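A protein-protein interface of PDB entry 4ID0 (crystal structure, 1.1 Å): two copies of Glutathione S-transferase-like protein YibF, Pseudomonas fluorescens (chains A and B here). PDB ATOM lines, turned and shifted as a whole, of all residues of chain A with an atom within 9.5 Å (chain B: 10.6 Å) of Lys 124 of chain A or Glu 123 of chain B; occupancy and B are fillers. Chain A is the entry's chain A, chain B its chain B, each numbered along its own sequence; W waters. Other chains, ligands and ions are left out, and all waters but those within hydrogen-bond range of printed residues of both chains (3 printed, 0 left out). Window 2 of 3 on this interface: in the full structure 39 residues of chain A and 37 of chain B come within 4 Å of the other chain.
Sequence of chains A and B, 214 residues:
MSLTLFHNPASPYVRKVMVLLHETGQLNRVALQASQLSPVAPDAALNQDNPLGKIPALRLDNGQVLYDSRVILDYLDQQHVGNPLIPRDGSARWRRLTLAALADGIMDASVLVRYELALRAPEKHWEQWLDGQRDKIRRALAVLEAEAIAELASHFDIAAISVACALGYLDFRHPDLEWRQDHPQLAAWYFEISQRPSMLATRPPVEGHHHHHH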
ATOM      1  N   GLU A 116       7.600 -17.527 -28.602  1.00  0.00           N
ATOM      2  CA  GLU A 116       7.362 -18.934 -28.353  1.00  0.00           C
ATOM      3  C   GLU A 116       8.269 -19.777 -29.231  1.00  0.00           C
ATOM      4  O   GLU A 116       8.906 -20.736 -28.725  1.00  0.00           O
ATOM      5  CB  GLU A 116       5.887 -19.254 -28.605  1.00  0.00           C
ATOM      6  CG  GLU A 116       5.634 -20.765 -28.368  1.00  0.00           C
ATOM      7  CD  GLU A 116       4.197 -21.140 -28.040  1.00  0.00           C
ATOM      8  OE1 GLU A 116       3.375 -20.273 -27.672  1.00  0.00           O
ATOM      9  OE2 GLU A 116       3.903 -22.362 -28.098  1.00  0.00           O
ATOM     10  N   LEU A 117       8.279 -19.509 -30.528  1.00  0.00           N
ATOM     11  CA  LEU A 117       9.072 -20.326 -31.450  1.00  0.00           C
ATOM     12  C   LEU A 117      10.553 -20.265 -31.144  1.00  0.00           C
ATOM     13  O   LEU A 117      11.264 -21.310 -31.196  1.00  0.00           O
ATOM     14  CB  LEU A 117       8.812 -19.958 -32.893  1.00  0.00           C
ATOM     15  CG  LEU A 117       7.409 -20.326 -33.390  1.00  0.00           C
ATOM     16  CD1 LEU A 117       7.222 -19.858 -34.840  1.00  0.00           C
ATOM     17  CD2 LEU A 117       7.126 -21.841 -33.285  1.00  0.00           C
ATOM     18  N   LEU A 119      12.140 -19.255 -28.204  1.00  0.00           N
ATOM     19  CA  LEU A 119      12.586 -19.413 -26.839  1.00  0.00           C
ATOM     20  C   LEU A 119      12.029 -20.590 -26.066  1.00  0.00           C
ATOM     21  O   LEU A 119      12.675 -21.123 -25.206  1.00  0.00           O
ATOM     22  CB  LEU A 119      12.360 -18.134 -26.054  1.00  0.00           C
ATOM     23  CG  LEU A 119      12.978 -16.867 -26.634  1.00  0.00           C
ATOM     24  CD1 LEU A 119      12.530 -15.651 -25.807  1.00  0.00           C
ATOM     25  CD2 LEU A 119      14.470 -16.922 -26.844  1.00  0.00           C
ATOM     26  N   ARG A 120      10.779 -20.970 -26.373  1.00  0.00           N
ATOM     27  CA  ARG A 120      10.189 -22.091 -25.678  1.00  0.00           C
ATOM     28  C   ARG A 120      10.662 -23.411 -26.325  1.00  0.00           C
ATOM     29  O   ARG A 120      10.848 -23.463 -27.552  1.00  0.00           O
ATOM     30  CB  ARG A 120       8.655 -22.014 -25.725  1.00  0.00           C
ATOM     31  CG  ARG A 120       7.949 -23.107 -24.950  1.00  0.00           C
ATOM     32  CD  ARG A 120       6.400 -22.933 -24.966  1.00  0.00           C
ATOM     33  NE  ARG A 120       6.000 -21.708 -24.249  1.00  0.00           N
ATOM     34  CZ  ARG A 120       5.191 -21.645 -23.179  1.00  0.00           C
ATOM     35  NH1 ARG A 120       4.633 -22.714 -22.652  1.00  0.00           N
ATOM     36  NH2 ARG A 120       4.976 -20.459 -22.645  1.00  0.00           N
ATOM     37  N   ALA A 121      10.859 -24.434 -25.525  1.00  0.00           N
ATOM     38  CA  ALA A 121      11.267 -25.745 -26.047  1.00  0.00           C
ATOM     39  C   ALA A 121      10.281 -26.221 -27.125  1.00  0.00           C
ATOM     40  O   ALA A 121       9.080 -26.101 -26.954  1.00  0.00           O
ATOM     41  CB  ALA A 121      11.272 -26.722 -24.919  1.00  0.00           C
ATOM     42  N   PRO A 122      10.779 -26.820 -28.228  1.00  0.00           N
ATOM     43  CA  PRO A 122       9.863 -27.258 -29.296  1.00  0.00           C
ATOM     44  C   PRO A 122       8.780 -28.180 -28.836  1.00  0.00           C
ATOM     45  O   PRO A 122       7.652 -28.087 -29.359  1.00  0.00           O
ATOM     46  CB  PRO A 122      10.798 -27.937 -30.318  1.00  0.00           C
ATOM     47  CG  PRO A 122      12.067 -27.096 -30.167  1.00  0.00           C
ATOM     48  CD  PRO A 122      12.182 -26.906 -28.652  1.00  0.00           C
ATOM     49  N   GLU A 123       9.068 -29.072 -27.903  1.00  0.00           N
ATOM     50  CA  GLU A 123       8.083 -30.023 -27.440  1.00  0.00           C
ATOM     51  C   GLU A 123       6.939 -29.324 -26.709  1.00  0.00           C
ATOM     52  O   GLU A 123       5.849 -29.917 -26.547  1.00  0.00           O
ATOM     53  CB  GLU A 123       8.763 -31.045 -26.516  1.00  0.00           C
ATOM     54  CG  GLU A 123       9.966 -31.748 -27.138  1.00  0.00           C
ATOM     55  CD  GLU A 123      11.300 -31.114 -26.757  1.00  0.00           C
ATOM     56  OE1 GLU A 123      11.464 -29.873 -26.699  1.00  0.00           O
ATOM     57  OE2 GLU A 123      12.234 -31.921 -26.505  1.00  0.00           O
ATOM     58  N   LYS A 124       7.170 -28.084 -26.273  1.00  0.00           N
ATOM     59  CA  LYS A 124       6.127 -27.317 -25.567  1.00  0.00           C
ATOM     60  C   LYS A 124       5.423 -26.290 -26.439  1.00  0.00           C
ATOM     61  O   LYS A 124       4.568 -25.548 -25.972  1.00  0.00           O
ATOM     62  CB  LYS A 124       6.679 -26.671 -24.315  1.00  0.00           C
ATOM     63  CG  LYS A 124       7.263 -27.685 -23.317  1.00  0.00           C
ATOM     64  CD  LYS A 124       7.682 -27.009 -22.019  1.00  0.00           C
ATOM     65  CE  LYS A 124       7.986 -28.051 -20.915  1.00  0.00           C
ATOM     66  NZ  LYS A 124       8.428 -27.343 -19.662  1.00  0.00           N
ATOM     67  N   HIS A 125       5.794 -26.214 -27.719  1.00  0.00           N
ATOM     68  CA  HIS A 125       5.067 -25.357 -28.649  1.00  0.00           C
ATOM     69  C   HIS A 125       3.676 -25.874 -28.796  1.00  0.00           C
ATOM     70  O   HIS A 125       3.449 -27.092 -28.805  1.00  0.00           O
ATOM     71  CB  HIS A 125       5.751 -25.328 -30.015  1.00  0.00           C
ATOM     72  CG  HIS A 125       7.113 -24.691 -30.014  1.00  0.00           C
ATOM     73  ND1 HIS A 125       7.876 -24.653 -31.156  1.00  0.00           N
ATOM     74  CD2 HIS A 125       7.844 -24.108 -29.027  1.00  0.00           C
ATOM     75  CE1 HIS A 125       9.023 -24.062 -30.882  1.00  0.00           C
ATOM     76  NE2 HIS A 125       9.025 -23.717 -29.604  1.00  0.00           N
ATOM     77  N   TRP A 126       2.725 -24.950 -28.912  1.00  0.00           N
ATOM     78  CA  TRP A 126       1.299 -25.289 -29.053  1.00  0.00           C
ATOM     79  C   TRP A 126       0.796 -24.733 -30.372  1.00  0.00           C
ATOM     80  O   TRP A 126       0.565 -23.540 -30.513  1.00  0.00           O
ATOM     81  CB  TRP A 126       0.516 -24.721 -27.879  1.00  0.00           C
ATOM     82  CG  TRP A 126      -0.955 -25.079 -27.916  1.00  0.00           C
ATOM     83  CD1 TRP A 126      -1.544 -26.068 -28.686  1.00  0.00           C
ATOM     84  CD2 TRP A 126      -1.988 -24.496 -27.131  1.00  0.00           C
ATOM     85  NE1 TRP A 126      -2.905 -26.099 -28.432  1.00  0.00           N
ATOM     86  CE2 TRP A 126      -3.196 -25.157 -27.476  1.00  0.00           C
ATOM     87  CE3 TRP A 126      -2.012 -23.502 -26.159  1.00  0.00           C
ATOM     88  CZ2 TRP A 126      -4.424 -24.801 -26.897  1.00  0.00           C
ATOM     89  CZ3 TRP A 126      -3.221 -23.141 -25.604  1.00  0.00           C
ATOM     90  CH2 TRP A 126      -4.417 -23.828 -25.942  1.00  0.00           C
ATOM     91  N   GLU A 127       0.692 -25.608 -31.373  1.00  0.00           N
ATOM     92  CA  GLU A 127       0.493 -25.153 -32.741  1.00  0.00           C
ATOM     93  C   GLU A 127      -0.861 -24.479 -32.911  1.00  0.00           C
ATOM     94  O   GLU A 127      -0.973 -23.499 -33.676  1.00  0.00           O
ATOM     95  CB  GLU A 127       0.691 -26.302 -33.741  1.00  0.00           C
ATOM     96  CG  GLU A 127       0.782 -25.825 -35.200  1.00  0.00           C
ATOM     97  CD  GLU A 127       1.962 -24.954 -35.531  1.00  0.00           C
ATOM     98  OE1 GLU A 127       2.903 -24.857 -34.686  1.00  0.00           O
ATOM     99  OE2 GLU A 127       2.000 -24.325 -36.625  1.00  0.00           O
ATOM    100  N   GLN A 128      -1.900 -24.954 -32.237  1.00  0.00           N
ATOM    101  CA  GLN A 128      -3.212 -24.317 -32.395  1.00  0.00           C
ATOM    102  C   GLN A 128      -3.188 -22.907 -31.805  1.00  0.00           C
ATOM    103  O   GLN A 128      -3.863 -21.992 -32.327  1.00  0.00           O
ATOM    104  CB  GLN A 128      -4.304 -25.144 -31.717  1.00  0.00           C
ATOM    105  CG  GLN A 128      -4.625 -26.482 -32.350  1.00  0.00           C
ATOM    106  CD  GLN A 128      -3.590 -27.568 -32.038  1.00  0.00           C
ATOM    107  OE1 GLN A 128      -2.692 -27.437 -31.218  1.00  0.00           O
ATOM    108  NE2 GLN A 128      -3.753 -28.708 -32.725  1.00  0.00           N
ATOM    109  N   TRP A 129      -2.436 -22.692 -30.733  1.00  0.00           N
ATOM    110  CA  TRP A 129      -2.246 -21.352 -30.198  1.00  0.00           C
ATOM    111  C   TRP A 129      -1.503 -20.468 -31.195  1.00  0.00           C
ATOM    112  O   TRP A 129      -1.914 -19.326 -31.474  1.00  0.00           O
ATOM    113  CB  TRP A 129      -1.459 -21.441 -28.897  1.00  0.00           C
ATOM    114  CG  TRP A 129      -1.045 -20.122 -28.314  1.00  0.00           C
ATOM    115  CD1 TRP A 129       0.129 -19.462 -28.552  1.00  0.00           C
ATOM    116  CD2 TRP A 129      -1.770 -19.311 -27.384  1.00  0.00           C
ATOM    117  NE1 TRP A 129       0.165 -18.289 -27.859  1.00  0.00           N
ATOM    118  CE2 TRP A 129      -0.973 -18.177 -27.119  1.00  0.00           C
ATOM    119  CE3 TRP A 129      -2.988 -19.460 -26.731  1.00  0.00           C
ATOM    120  CZ2 TRP A 129      -1.384 -17.176 -26.225  1.00  0.00           C
ATOM    121  CZ3 TRP A 129      -3.384 -18.455 -25.841  1.00  0.00           C
ATOM    122  CH2 TRP A 129      -2.580 -17.341 -25.607  1.00  0.00           C
ATOM    123  N   LEU A 130      -0.384 -20.965 -31.707  1.00  0.00           N
ATOM    124  CA  LEU A 130       0.379 -20.216 -32.694  1.00  0.00           C
ATOM    125  C   LEU A 130      -0.470 -19.880 -33.924  1.00  0.00           C
ATOM    126  O   LEU A 130      -0.418 -18.734 -34.410  1.00  0.00           O
ATOM    127  CB  LEU A 130       1.632 -21.004 -33.085  1.00  0.00           C
ATOM    128  CG  LEU A 130       2.585 -21.175 -31.898  1.00  0.00           C
ATOM    129  CD1 LEU A 130       3.613 -22.298 -32.238  1.00  0.00           C
ATOM    130  CD2 LEU A 130       3.342 -19.910 -31.539  1.00  0.00           C
ATOM    131  N   GLU B 116      -2.220 -19.544 -20.453  1.00  0.00           N
ATOM    132  CA  GLU B 116      -1.323 -20.682 -20.369  1.00  0.00           C
ATOM    133  C   GLU B 116      -1.845 -21.678 -19.348  1.00  0.00           C
ATOM    134  O   GLU B 116      -1.937 -22.899 -19.626  1.00  0.00           O
ATOM    135  CB  GLU B 116       0.062 -20.188 -19.964  1.00  0.00           C
ATOM    136  CG  GLU B 116       1.054 -21.371 -19.750  1.00  0.00           C
ATOM    137  CD  GLU B 116       2.316 -21.320 -20.552  1.00  0.00           C
ATOM    138  OE1 GLU B 116       2.375 -20.508 -21.461  1.00  0.00           O
ATOM    139  OE2 GLU B 116       3.197 -22.162 -20.288  1.00  0.00           O
ATOM    140  N   LEU B 117      -2.188 -21.203 -18.150  1.00  0.00           N
ATOM    141  CA  LEU B 117      -2.610 -22.132 -17.109  1.00  0.00           C
ATOM    142  C   LEU B 117      -3.925 -22.822 -17.400  1.00  0.00           C
ATOM    143  O   LEU B 117      -4.100 -23.996 -17.081  1.00  0.00           O
ATOM    144  CB  LEU B 117      -2.678 -21.419 -15.784  1.00  0.00           C
ATOM    145  CG  LEU B 117      -1.354 -20.908 -15.242  1.00  0.00           C
ATOM    146  CD1 LEU B 117      -1.601 -20.122 -13.973  1.00  0.00           C
ATOM    147  CD2 LEU B 117      -0.363 -22.034 -14.985  1.00  0.00           C
ATOM    148  N   LEU B 119      -5.674 -23.018 -20.519  1.00  0.00           N
ATOM    149  CA  LEU B 119      -5.926 -23.562 -21.841  1.00  0.00           C
ATOM    150  C   LEU B 119      -4.819 -24.480 -22.355  1.00  0.00           C
ATOM    151  O   LEU B 119      -5.089 -25.425 -23.058  1.00  0.00           O
ATOM    152  CB  LEU B 119      -6.165 -22.446 -22.856  1.00  0.00           C
ATOM    153  CG  LEU B 119      -7.264 -21.435 -22.489  1.00  0.00           C
ATOM    154  CD1 LEU B 119      -7.416 -20.419 -23.624  1.00  0.00           C
ATOM    155  CD2 LEU B 119      -8.613 -22.074 -22.104  1.00  0.00           C
ATOM    156  N   ARG B 120      -3.560 -24.152 -22.074  1.00  0.00           N
ATOM    157  CA  ARG B 120      -2.452 -24.948 -22.615  1.00  0.00           C
ATOM    158  C   ARG B 120      -2.322 -26.252 -21.833  1.00  0.00           C
ATOM    159  O   ARG B 120      -2.469 -26.275 -20.597  1.00  0.00           O
ATOM    160  CB  ARG B 120      -1.160 -24.123 -22.553  1.00  0.00           C
ATOM    161  CG  ARG B 120       0.043 -24.833 -23.191  1.00  0.00           C
ATOM    162  CD  ARG B 120       1.292 -23.958 -23.234  1.00  0.00           C
ATOM    163  NE  ARG B 120       1.089 -22.792 -24.099  1.00  0.00           N
ATOM    164  CZ  ARG B 120       1.789 -22.501 -25.188  1.00  0.00           C
ATOM    165  NH1 ARG B 120       2.808 -23.226 -25.631  1.00  0.00           N
ATOM    166  NH2 ARG B 120       1.456 -21.431 -25.905  1.00  0.00           N
ATOM    167  N   ALA B 121      -2.035 -27.337 -22.537  1.00  0.00           N
ATOM    168  CA  ALA B 121      -1.831 -28.641 -21.881  1.00  0.00           C
ATOM    169  C   ALA B 121      -0.748 -28.492 -20.801  1.00  0.00           C
ATOM    170  O   ALA B 121       0.301 -27.889 -21.043  1.00  0.00           O
ATOM    171  CB  ALA B 121      -1.392 -29.659 -22.894  1.00  0.00           C
ATOM    172  N   PRO B 122      -0.964 -29.091 -19.608  1.00  0.00           N
ATOM    173  CA  PRO B 122       0.046 -28.923 -18.539  1.00  0.00           C
ATOM    174  C   PRO B 122       1.448 -29.377 -18.926  1.00  0.00           C
ATOM    175  O   PRO B 122       2.386 -28.743 -18.461  1.00  0.00           O
ATOM    176  CB  PRO B 122      -0.507 -29.771 -17.388  1.00  0.00           C
ATOM    177  CG  PRO B 122      -1.971 -29.868 -17.619  1.00  0.00           C
ATOM    178  CD  PRO B 122      -2.218 -29.701 -19.114  1.00  0.00           C
ATOM    179  N   GLU B 123       1.597 -30.389 -19.762  1.00  0.00           N
ATOM    180  CA  GLU B 123       2.937 -30.829 -20.110  1.00  0.00           C
ATOM    181  C   GLU B 123       3.671 -29.799 -20.954  1.00  0.00           C
ATOM    182  O   GLU B 123       4.897 -29.875 -21.096  1.00  0.00           O
ATOM    183  CB  GLU B 123       2.864 -32.180 -20.842  1.00  0.00           C
ATOM    184  CG  GLU B 123       1.946 -32.196 -22.094  1.00  0.00           C
ATOM    185  CD  GLU B 123       0.448 -32.479 -21.824  1.00  0.00           C
ATOM    186  OE1 GLU B 123      -0.103 -32.262 -20.690  1.00  0.00           O
ATOM    187  OE2 GLU B 123      -0.203 -33.012 -22.772  1.00  0.00           O
ATOM    188  N   LYS B 124       2.934 -28.857 -21.528  1.00  0.00           N
ATOM    189  CA  LYS B 124       3.539 -27.775 -22.315  1.00  0.00           C
ATOM    190  C   LYS B 124       3.692 -26.453 -21.556  1.00  0.00           C
ATOM    191  O   LYS B 124       4.169 -25.473 -22.115  1.00  0.00           O
ATOM    192  CB  LYS B 124       2.770 -27.562 -23.601  1.00  0.00           C
ATOM    193  CG  LYS B 124       2.797 -28.810 -24.514  1.00  0.00           C
ATOM    194  CD  LYS B 124       2.199 -28.506 -25.873  1.00  0.00           C
ATOM    195  CE  LYS B 124       2.407 -29.696 -26.815  1.00  0.00           C
ATOM    196  NZ  LYS B 124       1.749 -29.441 -28.121  1.00  0.00           N
ATOM    197  N   HIS B 125       3.376 -26.444 -20.264  1.00  0.00           N
ATOM    198  CA  HIS B 125       3.586 -25.235 -19.478  1.00  0.00           C
ATOM    199  C   HIS B 125       5.087 -25.027 -19.352  1.00  0.00           C
ATOM    200  O   HIS B 125       5.866 -25.989 -19.241  1.00  0.00           O
ATOM    201  CB  HIS B 125       2.982 -25.337 -18.074  1.00  0.00           C
ATOM    202  CG  HIS B 125       1.483 -25.348 -18.072  1.00  0.00           C
ATOM    203  ND1 HIS B 125       0.736 -25.424 -16.914  1.00  0.00           N
ATOM    204  CD2 HIS B 125       0.600 -25.315 -19.096  1.00  0.00           C
ATOM    205  CE1 HIS B 125      -0.549 -25.432 -17.238  1.00  0.00           C
ATOM    206  NE2 HIS B 125      -0.658 -25.377 -18.548  1.00  0.00           N
ATOM    207  N   TRP B 126       5.476 -23.767 -19.350  1.00  0.00           N
ATOM    208  CA  TRP B 126       6.881 -23.424 -19.171  1.00  0.00           C
ATOM    209  C   TRP B 126       7.040 -22.556 -17.939  1.00  0.00           C
ATOM    210  O   TRP B 126       6.665 -21.379 -17.919  1.00  0.00           O
ATOM    211  CB  TRP B 126       7.405 -22.707 -20.411  1.00  0.00           C
ATOM    212  CG  TRP B 126       8.882 -22.393 -20.343  1.00  0.00           C
ATOM    213  CD1 TRP B 126       9.810 -22.919 -19.497  1.00  0.00           C
ATOM    214  CD2 TRP B 126       9.571 -21.474 -21.177  1.00  0.00           C
ATOM    215  NE1 TRP B 126      11.051 -22.397 -19.777  1.00  0.00           N
ATOM    216  CE2 TRP B 126      10.922 -21.472 -20.777  1.00  0.00           C
ATOM    217  CE3 TRP B 126       9.173 -20.636 -22.223  1.00  0.00           C
ATOM    218  CZ2 TRP B 126      11.880 -20.662 -21.385  1.00  0.00           C
ATOM    219  CZ3 TRP B 126      10.119 -19.803 -22.809  1.00  0.00           C
ATOM    220  CH2 TRP B 126      11.450 -19.828 -22.386  1.00  0.00           C
ATOM    221  N   GLU B 127       7.531 -23.167 -16.869  1.00  0.00           N
ATOM    222  CA  GLU B 127       7.530 -22.506 -15.552  1.00  0.00           C
ATOM    223  C   GLU B 127       8.357 -21.250 -15.552  1.00  0.00           C
ATOM    224  O   GLU B 127       7.976 -20.253 -14.918  1.00  0.00           O
ATOM    225  CB  GLU B 127       7.984 -23.457 -14.453  1.00  0.00           C
ATOM    226  CG  GLU B 127       7.016 -24.597 -14.313  1.00  0.00           C
ATOM    227  CD  GLU B 127       5.570 -24.162 -14.078  1.00  0.00           C
ATOM    228  OE1 GLU B 127       5.364 -23.210 -13.263  1.00  0.00           O
ATOM    229  OE2 GLU B 127       4.660 -24.784 -14.710  1.00  0.00           O
ATOM    230  N   GLN B 128       9.496 -21.244 -16.232  1.00  0.00           N
ATOM    231  CA  GLN B 128      10.331 -20.034 -16.220  1.00  0.00           C
ATOM    232  C   GLN B 128       9.590 -18.899 -16.940  1.00  0.00           C
ATOM    233  O   GLN B 128       9.737 -17.737 -16.554  1.00  0.00           O
ATOM    234  CB  GLN B 128      11.647 -20.295 -16.920  1.00  0.00           C
ATOM    235  CG  GLN B 128      12.595 -21.134 -16.117  1.00  0.00           C
ATOM    236  CD  GLN B 128      12.322 -22.646 -16.092  1.00  0.00           C
ATOM    237  OE1 GLN B 128      11.412 -23.229 -16.739  1.00  0.00           O
ATOM    238  NE2 GLN B 128      13.189 -23.320 -15.347  1.00  0.00           N
ATOM    239  N   TRP B 129       8.821 -19.209 -17.981  1.00  0.00           N
ATOM    240  CA  TRP B 129       8.009 -18.199 -18.647  1.00  0.00           C
ATOM    241  C   TRP B 129       6.929 -17.666 -17.717  1.00  0.00           C
ATOM    242  O   TRP B 129       6.702 -16.435 -17.607  1.00  0.00           O
ATOM    243  CB  TRP B 129       7.441 -18.771 -19.951  1.00  0.00           C
ATOM    244  CG  TRP B 129       6.573 -17.806 -20.665  1.00  0.00           C
ATOM    245  CD1 TRP B 129       6.929 -16.973 -21.677  1.00  0.00           C
ATOM    246  CD2 TRP B 129       5.168 -17.611 -20.444  1.00  0.00           C
ATOM    247  NE1 TRP B 129       5.820 -16.216 -22.055  1.00  0.00           N
ATOM    248  CE2 TRP B 129       4.737 -16.603 -21.317  1.00  0.00           C
ATOM    249  CE3 TRP B 129       4.232 -18.167 -19.567  1.00  0.00           C
ATOM    250  CZ2 TRP B 129       3.393 -16.143 -21.343  1.00  0.00           C
ATOM    251  CZ3 TRP B 129       2.902 -17.693 -19.578  1.00  0.00           C
ATOM    252  CH2 TRP B 129       2.497 -16.723 -20.461  1.00  0.00           C
ATOM    253  N   LEU B 130       6.258 -18.572 -17.036  1.00  0.00           N
ATOM    254  CA  LEU B 130       5.200 -18.177 -16.107  1.00  0.00           C
ATOM    255  C   LEU B 130       5.755 -17.309 -15.011  1.00  0.00           C
ATOM    256  O   LEU B 130       5.170 -16.259 -14.686  1.00  0.00           O
ATOM    257  CB  LEU B 130       4.537 -19.435 -15.548  1.00  0.00           C
ATOM    258  CG  LEU B 130       3.582 -20.174 -16.492  1.00  0.00           C
ATOM    259  CD1 LEU B 130       3.318 -21.573 -15.965  1.00  0.00           C
ATOM    260  CD2 LEU B 130       2.241 -19.417 -16.605  1.00  0.00           C
HETATM  261  O   HOH W   1       8.509 -25.797 -17.163  1.00  0.00           O
HETATM  262  O   HOH W   2       1.041 -28.383 -30.784  1.00  0.00           O
HETATM  263  O   HOH W   3      10.707 -24.202 -22.627  1.00  0.00           O
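NE1 of Trp 126 of chain A sits at hydrogen-bond distance from OE1 of Gln 128 of chain A (3.1 Å).
A ring nitrogen (NE2) of His 125 of chain B lies within hydrogen-bond range of the backbone carbonyl oxygen (O) of Glu 116 of chain B, 3.0 Å away.
NE2 of His 125 of chain A lies within hydrogen-bond range of O of Glu 116 of chain A (3.1 Å).
The backbone carbonyl oxygen (O) of Arg 120 of chain B is in hydrogen-bond range of a ring nitrogen (NE2) of His 125 of chain B (2.9 Å).
The indole nitrogen (NE1) of Trp 126 of chain B sits at hydrogen-bond distance from the side-chain amide oxygen (OE1) of Gln 128 of chain B, at 3.2 Å.
The backbone NH of Trp 126 of chain A lies within hydrogen-bond range of the side-chain carboxylate of Glu 116 of chain A (3.0 Å).
Arg 120 of chain A touches Lys 124 of chain B, and with the chains exchanged Lys 124 of chain A touches Arg 120 of chain B.
Arg 120 of chain A touches Trp 129 of chain B, and with the chains exchanged Trp 129 of chain A touches Arg 120 of chain B.
Glu 123 of chain A touches Lys 124 of chain B, and with the chains exchanged Lys 124 of chain A touches Glu 123 of chain B.
Lys 124 of chain A touches His 125 of chain B, and with the chains exchanged His 125 of chain A touches Lys 124 of chain B.
Of the printed residues of chain B, Arg 120 of chain A touches Glu 116 (2.8 Å), Arg 120 (3.5 Å), Lys 124 (2.8 Å), Trp 126 (3.6 Å) and Trp 129 (3.6 Å).
No residue of chain B comes within 4 Å of Pro 122 of chain A.
Printed residues of chain B within 4 Å of Lys 124 of chain A: Arg 120, Glu 123, Lys 124 and His 125.
Of chain B, only Lys 124 comes within 4 Å of His 125 of chain A.
Gln 128 of chain A touches none of the printed residues of chain B.
Of chain A, only Lys 124 (3.6 Å) comes within 4 Å of Glu 123 of chain B.
Of the printed residues of chain A, Trp 129 of chain B touches Arg 120.
Leu 130 of chain B touches none of the printed residues of chain A.
The nearest residue of chain B that does not touch Lys 124 of chain A is Trp 126 of chain B (4.2 Å).
The nearest printed residue of chain A that does not touch Glu 123 of chain B is Glu 123 of chain A (5.5 Å).
O of Leu 119 of chain A touches CH2 of Trp 126 of chain B, at 3.3 Å.
Arg 120 of chain A touches Arg 120 of chain B.
CB of Trp 126 of chain B touches NH1 of Arg 120 of chain A, at 3.6 Å.
NH2 of Arg 120 of chain A touches CD2 of Trp 129 of chain B, at 3.6 Å.
CE of Lys 124 of chain B touches O of Glu 123 of chain A (3.5 Å).
Glu 123 of chain B touches Lys 124 of chain A.
Lys 124 of chain A touches Lys 124 of chain B (CB to O, 3.5 Å).
Leu 119 of chain B touches Trp 126 of chain A (O to CH2, 3.4 Å).
Trp 126 of chain A touches Arg 120 of chain B (CB to NH1, 3.5 Å).
Arg 120 of chain B touches Trp 129 of chain A (NH2 to CD1, 3.6 Å).
NH1 of Arg 120 of chain B is in hydrogen-bond range of O of Lys 124 of chain A.
The backbone carbonyl oxygen (O) of His 125 of chain A sits at hydrogen-bond distance from the side-chain amino group (NZ) of Lys 124 of chain B.
NH1 of Arg 120 of chain A sits at hydrogen-bond distance from O of Lys 124 of chain B (2.8 Å).
The guanidinium group (NH1) of Arg 120 of chain A is in salt-bridge range of the side-chain carboxylate (OE2) of Glu 116 of chain B (2.8 Å).
The side-chain carboxylate (OE2) of Glu 116 of chain A lies within salt-bridge range of the guanidinium group (NH1) of Arg 120 of chain B (2.8 Å).
NZ of Lys 124 of chain A is in hydrogen-bond range of O of His 125 of chain B, at 2.9 Å.
Water W1 lies within hydrogen-bond range of the backbone NH of Glu 127 of chain B (2.8 Å), the side-chain amino group of Lys 124 of chain A (2.9 Å) and the backbone carbonyl oxygen of His 125 of chain B (3.4 Å).
Water W2 lies within hydrogen-bond range of the backbone NH of Glu 127 of chain A (2.9 Å), the side-chain amino group of Lys 124 of chain B (3.0 Å) and the backbone carbonyl oxygen of His 125 of chain A (3.4 Å).
Water W3 lies within hydrogen-bond range of N of Ala 121 of chain A and NE1 of Trp 126 of chain B.
Of the 14 printed residues of chain B, 8 touch a printed residue of chain A.
Printed residues of chain A that touch a printed residue of chain B: Glu 116, Leu 119, Arg 120, Glu 123, Lys 124, His 125, Trp 126 and Trp 129.
Hydrophobic or aromatic side chains of chain A within 4 Å of the printed part of chain B: Trp 126 and Trp 129.
Along chain A the printed residues that touch a printed residue of chain B span positions 116 to 129.
Among the printed residues, Asp or Glu carboxylates within 4 Å of a Lys or Arg side-chain nitrogen of the other chain: Glu 116 of chain A with Arg 120 of chain B (2.8 Å) and Arg 120 of chain A with Glu 116 of chain B (2.8 Å).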
